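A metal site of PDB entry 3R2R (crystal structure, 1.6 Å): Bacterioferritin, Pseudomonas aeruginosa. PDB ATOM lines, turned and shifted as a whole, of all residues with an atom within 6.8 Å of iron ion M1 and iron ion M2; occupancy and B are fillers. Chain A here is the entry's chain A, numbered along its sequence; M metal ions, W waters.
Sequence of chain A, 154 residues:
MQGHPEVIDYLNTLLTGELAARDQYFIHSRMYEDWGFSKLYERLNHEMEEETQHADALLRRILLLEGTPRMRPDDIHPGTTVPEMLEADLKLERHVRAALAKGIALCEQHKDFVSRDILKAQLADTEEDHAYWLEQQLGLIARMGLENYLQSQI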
ATOM      1  N   GLY A  17     -24.377  13.981  24.199  1.00  0.00           N
ATOM      2  CA  GLY A  17     -23.098  13.465  24.690  1.00  0.00           C
ATOM      3  C   GLY A  17     -22.466  14.453  25.683  1.00  0.00           C
ATOM      4  O   GLY A  17     -21.894  14.070  26.693  1.00  0.00           O
ATOM      5  N   GLU A  18     -22.523  15.754  25.387  1.00  0.00           N
ATOM      6  CA  GLU A  18     -21.909  16.746  26.290  1.00  0.00           C
ATOM      7  C   GLU A  18     -22.706  16.934  27.591  1.00  0.00           C
ATOM      8  O   GLU A  18     -22.125  17.121  28.670  1.00  0.00           O
ATOM      9  CB  GLU A  18     -21.758  18.106  25.597  1.00  0.00           C
ATOM     10  CG  GLU A  18     -20.867  18.035  24.365  1.00  0.00           C
ATOM     11  CD  GLU A  18     -19.463  17.559  24.709  1.00  0.00           C
ATOM     12  OE1 GLU A  18     -18.885  18.084  25.681  1.00  0.00           O
ATOM     13  OE2 GLU A  18     -18.959  16.692  23.958  1.00  0.00           O
ATOM     14  N   ALA A  21     -21.584  14.077  29.654  1.00  0.00           N
ATOM     15  CA  ALA A  21     -20.228  14.293  30.234  1.00  0.00           C
ATOM     16  C   ALA A  21     -20.352  15.222  31.460  1.00  0.00           C
ATOM     17  O   ALA A  21     -19.791  14.931  32.525  1.00  0.00           O
ATOM     18  CB  ALA A  21     -19.296  14.881  29.172  1.00  0.00           C
ATOM     19  N   TYR A  25     -19.434  14.009  35.336  1.00  0.00           N
ATOM     20  CA  TYR A  25     -18.498  14.748  36.197  1.00  0.00           C
ATOM     21  C   TYR A  25     -19.201  15.329  37.448  1.00  0.00           C
ATOM     22  O   TYR A  25     -18.579  15.482  38.527  1.00  0.00           O
ATOM     23  CB  TYR A  25     -17.825  15.869  35.394  1.00  0.00           C
ATOM     24  CG  TYR A  25     -16.868  15.321  34.359  1.00  0.00           C
ATOM     25  CD1 TYR A  25     -16.038  14.253  34.667  1.00  0.00           C
ATOM     26  CD2 TYR A  25     -16.751  15.894  33.116  1.00  0.00           C
ATOM     27  CE1 TYR A  25     -15.117  13.755  33.740  1.00  0.00           C
ATOM     28  CE2 TYR A  25     -15.846  15.393  32.156  1.00  0.00           C
ATOM     29  CZ  TYR A  25     -15.052  14.321  32.490  1.00  0.00           C
ATOM     30  OH  TYR A  25     -14.143  13.833  31.579  1.00  0.00           O
ATOM     31  N   GLU A  47     -14.185  20.419  35.441  1.00  0.00           N
ATOM     32  CA  GLU A  47     -14.536  19.778  34.170  1.00  0.00           C
ATOM     33  C   GLU A  47     -16.059  19.810  33.951  1.00  0.00           C
ATOM     34  O   GLU A  47     -16.508  19.941  32.819  1.00  0.00           O
ATOM     35  CB  GLU A  47     -14.093  18.311  34.151  1.00  0.00           C
ATOM     36  CG  GLU A  47     -12.669  18.087  34.654  1.00  0.00           C
ATOM     37  CD  GLU A  47     -11.635  18.542  33.693  1.00  0.00           C
ATOM     38  OE1 GLU A  47     -10.812  17.691  33.253  1.00  0.00           O
ATOM     39  OE2 GLU A  47     -11.591  19.756  33.407  1.00  0.00           O
ATOM     40  N   GLU A  50     -16.736  23.005  32.477  1.00  0.00           N
ATOM     41  CA  GLU A  50     -16.280  23.000  31.089  1.00  0.00           C
ATOM     42  C   GLU A  50     -17.207  22.238  30.140  1.00  0.00           C
ATOM     43  O   GLU A  50     -17.483  22.716  29.037  1.00  0.00           O
ATOM     44  CB  GLU A  50     -14.877  22.453  30.992  1.00  0.00           C
ATOM     45  CG  GLU A  50     -13.918  23.487  31.632  1.00  0.00           C
ATOM     46  CD  GLU A  50     -12.480  23.095  31.514  1.00  0.00           C
ATOM     47  OE1 GLU A  50     -11.631  24.011  31.430  1.00  0.00           O
ATOM     48  OE2 GLU A  50     -12.188  21.883  31.543  1.00  0.00           O
ATOM     49  N   GLU A  51     -17.755  21.107  30.588  1.00  0.00           N
ATOM     50  CA  GLU A  51     -18.678  20.389  29.700  1.00  0.00           C
ATOM     51  C   GLU A  51     -19.986  21.170  29.570  1.00  0.00           C
ATOM     52  O   GLU A  51     -20.674  21.082  28.547  1.00  0.00           O
ATOM     53  CB  GLU A  51     -19.004  18.978  30.245  1.00  0.00           C
ATOM     54  CG  GLU A  51     -17.759  18.110  30.429  1.00  0.00           C
ATOM     55  CD  GLU A  51     -17.060  17.768  29.136  1.00  0.00           C
ATOM     56  OE1 GLU A  51     -17.411  18.279  28.095  1.00  0.00           O
ATOM     57  OE2 GLU A  51     -16.069  17.054  29.213  1.00  0.00           O
ATOM     58  N   HIS A  54     -19.309  23.425  26.863  1.00  0.00           N
ATOM     59  CA  HIS A  54     -19.316  22.697  25.567  1.00  0.00           C
ATOM     60  C   HIS A  54     -20.755  22.466  25.113  1.00  0.00           C
ATOM     61  O   HIS A  54     -21.073  22.674  23.954  1.00  0.00           O
ATOM     62  CB  HIS A  54     -18.650  21.337  25.715  1.00  0.00           C
ATOM     63  CG  HIS A  54     -17.159  21.403  25.722  1.00  0.00           C
ATOM     64  ND1 HIS A  54     -16.370  20.281  25.855  1.00  0.00           N
ATOM     65  CD2 HIS A  54     -16.318  22.457  25.614  1.00  0.00           C
ATOM     66  CE1 HIS A  54     -15.092  20.639  25.828  1.00  0.00           C
ATOM     67  NE2 HIS A  54     -15.033  21.952  25.670  1.00  0.00           N
ATOM     68  N   ALA A  55     -21.601  22.004  26.032  1.00  0.00           N
ATOM     69  CA  ALA A  55     -23.000  21.795  25.705  1.00  0.00           C
ATOM     70  C   ALA A  55     -23.646  23.102  25.255  1.00  0.00           C
ATOM     71  O   ALA A  55     -24.408  23.139  24.286  1.00  0.00           O
ATOM     72  CB  ALA A  55     -23.799  21.160  26.911  1.00  0.00           C
ATOM     73  N   LEU A  92     -15.325   7.727  28.469  1.00  0.00           N
ATOM     74  CA  LEU A  92     -16.247   8.778  28.061  1.00  0.00           C
ATOM     75  C   LEU A  92     -15.556   9.785  27.138  1.00  0.00           C
ATOM     76  O   LEU A  92     -16.060  10.155  26.096  1.00  0.00           O
ATOM     77  CB  LEU A  92     -16.778   9.494  29.323  1.00  0.00           C
ATOM     78  CG  LEU A  92     -17.780  10.624  29.090  1.00  0.00           C
ATOM     79  CD1 LEU A  92     -18.828  10.226  28.071  1.00  0.00           C
ATOM     80  CD2 LEU A  92     -18.438  10.982  30.407  1.00  0.00           C
ATOM     81  N   GLU A  93     -14.393  10.271  27.556  1.00  0.00           N
ATOM     82  CA  GLU A  93     -13.671  11.246  26.731  1.00  0.00           C
ATOM     83  C   GLU A  93     -13.216  10.648  25.406  1.00  0.00           C
ATOM     84  O   GLU A  93     -13.259  11.333  24.408  1.00  0.00           O
ATOM     85  CB  GLU A  93     -12.503  11.870  27.503  1.00  0.00           C
ATOM     86  CG  GLU A  93     -12.991  12.739  28.690  1.00  0.00           C
ATOM     87  CD  GLU A  93     -13.582  14.086  28.273  1.00  0.00           C
ATOM     88  OE1 GLU A  93     -13.304  14.585  27.155  1.00  0.00           O
ATOM     89  OE2 GLU A  93     -14.328  14.672  29.096  1.00  0.00           O
ATOM     90  N   VAL A  96     -16.318  10.756  23.241  1.00  0.00           N
ATOM     91  CA  VAL A  96     -16.511  12.132  22.777  1.00  0.00           C
ATOM     92  C   VAL A  96     -15.526  12.513  21.659  1.00  0.00           C
ATOM     93  O   VAL A  96     -15.905  13.122  20.638  1.00  0.00           O
ATOM     94  CB  VAL A  96     -16.358  13.106  23.955  1.00  0.00           C
ATOM     95  CG1 VAL A  96     -16.325  14.582  23.475  1.00  0.00           C
ATOM     96  CG2 VAL A  96     -17.496  12.892  24.968  1.00  0.00           C
ATOM     97  N   LEU A 100     -16.719  13.703  18.062  1.00  0.00           N
ATOM     98  CA  LEU A 100     -16.360  15.037  17.523  1.00  0.00           C
ATOM     99  C   LEU A 100     -15.626  14.939  16.165  1.00  0.00           C
ATOM    100  O   LEU A 100     -15.914  15.666  15.235  1.00  0.00           O
ATOM    101  CB  LEU A 100     -15.475  15.786  18.528  1.00  0.00           C
ATOM    102  CG  LEU A 100     -16.209  16.303  19.771  1.00  0.00           C
ATOM    103  CD1 LEU A 100     -15.131  16.754  20.786  1.00  0.00           C
ATOM    104  CD2 LEU A 100     -17.144  17.475  19.393  1.00  0.00           C
ATOM    105  N   GLN A 122     -13.679  22.141  20.694  1.00  0.00           N
ATOM    106  CA  GLN A 122     -13.984  21.139  21.714  1.00  0.00           C
ATOM    107  C   GLN A 122     -13.097  19.897  21.611  1.00  0.00           C
ATOM    108  O   GLN A 122     -12.769  19.271  22.624  1.00  0.00           O
ATOM    109  CB  GLN A 122     -15.455  20.698  21.615  1.00  0.00           C
ATOM    110  CG  GLN A 122     -16.361  21.843  21.877  1.00  0.00           C
ATOM    111  CD  GLN A 122     -17.774  21.420  22.194  1.00  0.00           C
ATOM    112  OE1 GLN A 122     -18.057  20.248  22.539  1.00  0.00           O
ATOM    113  NE2 GLN A 122     -18.675  22.378  22.118  1.00  0.00           N
ATOM    114  N   ASP A 125      -9.920  20.631  23.416  1.00  0.00           N
ATOM    115  CA  ASP A 125     -10.175  20.524  24.871  1.00  0.00           C
ATOM    116  C   ASP A 125     -10.227  19.073  25.295  1.00  0.00           C
ATOM    117  O   ASP A 125      -9.609  18.677  26.309  1.00  0.00           O
ATOM    118  CB  ASP A 125     -11.500  21.187  25.282  1.00  0.00           C
ATOM    119  CG  ASP A 125     -11.499  22.726  25.142  1.00  0.00           C
ATOM    120  OD1 ASP A 125     -10.400  23.339  25.031  1.00  0.00           O
ATOM    121  OD2 ASP A 125     -12.604  23.308  25.157  1.00  0.00           O
ATOM    122  N   THR A 126     -10.952  18.276  24.531  1.00  0.00           N
ATOM    123  CA  THR A 126     -11.114  16.846  24.858  1.00  0.00           C
ATOM    124  C   THR A 126      -9.768  16.114  24.850  1.00  0.00           C
ATOM    125  O   THR A 126      -9.443  15.382  25.777  1.00  0.00           O
ATOM    126  CB  THR A 126     -12.108  16.204  23.851  1.00  0.00           C
ATOM    127  OG1 THR A 126     -13.376  16.871  23.982  1.00  0.00           O
ATOM    128  CG2 THR A 126     -12.265  14.723  24.144  1.00  0.00           C
ATOM    129  N   HIS A 130      -8.919  17.290  28.836  1.00  0.00           N
ATOM    130  CA  HIS A 130      -9.770  16.334  29.577  1.00  0.00           C
ATOM    131  C   HIS A 130      -9.231  14.911  29.580  1.00  0.00           C
ATOM    132  O   HIS A 130      -9.001  14.314  30.654  1.00  0.00           O
ATOM    133  CB  HIS A 130     -11.183  16.303  29.004  1.00  0.00           C
ATOM    134  CG  HIS A 130     -11.908  17.589  29.178  1.00  0.00           C
ATOM    135  ND1 HIS A 130     -13.184  17.803  28.704  1.00  0.00           N
ATOM    136  CD2 HIS A 130     -11.543  18.737  29.803  1.00  0.00           C
ATOM    137  CE1 HIS A 130     -13.578  19.028  29.008  1.00  0.00           C
ATOM    138  NE2 HIS A 130     -12.595  19.623  29.685  1.00  0.00           N
ATOM    139  N   ALA A 131      -9.079  14.330  28.392  1.00  0.00           N
ATOM    140  CA  ALA A 131      -8.554  12.972  28.321  1.00  0.00           C
ATOM    141  C   ALA A 131      -7.105  12.934  28.831  1.00  0.00           C
ATOM    142  O   ALA A 131      -6.715  11.997  29.501  1.00  0.00           O
ATOM    143  CB  ALA A 131      -8.627  12.421  26.889  1.00  0.00           C
HETATM  144 FE    FE M   1     -16.888  18.190  25.992  1.00  0.00          FE
HETATM  145 FE    FE M   2     -14.656  16.382  27.929  1.00  0.00          FE
HETATM  146  O   HOH W   1     -16.673  18.124  23.770  1.00  0.00           O
HETATM  147  O   HOH W   2     -15.156  17.102  26.161  1.00  0.00           O
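The side-chain amide nitrogen (NE2) of Gln 122 sits at hydrogen-bond distance from the backbone carbonyl oxygen (O) of His 54, 3.0 Å away. OE2 of Glu 93 lies close to OH of Tyr 25 (2.6 Å). The backbone carbonyl oxygen (O) of Asp 125 sits at hydrogen-bond distance from the backbone NH (N) of His 130, 3.0 Å away. The side-chain carboxylate of Asp 125 is in hydrogen-bond range of a ring nitrogen (NE2) of His 54. The side-chain carboxylate of Glu 50 is in hydrogen-bond range of a ring nitrogen (NE2) of His 130 (3.0 Å).
Within 4 Å of iron ion M1: Glu 18, Glu 51 and His 54. The nearest printed residue that does not touch iron ion M1 is Gln 122 (4.2 Å).
The nearest printed residue that does not touch iron ion M2 is Thr 126 (4.2 Å).
OE1 of Glu 18 binds iron ion M1 (2.0 Å). Water W2 binds iron ion M1 (2.1 Å). ND1 of His 54 binds iron ion M1 (2.2 Å). Iron ion M1 is bound by OE1 of Glu 51. Water W1 is bound to iron ion M1 (2.2 Å).
Iron ion M2 is bound by water W2 (2.0 Å), the side-chain carboxylate (OE2) of Glu 51 (2.0 Å), the side-chain carboxylate (OE2) of Glu 93 (2.1 Å), a ring nitrogen (ND1) of His 130 (2.2 Å) and the side-chain carboxylate (OE1) of Glu 93 (2.4 Å).
Water W1 bridges OE2 of Glu 18 and OE1 of Gln 122.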
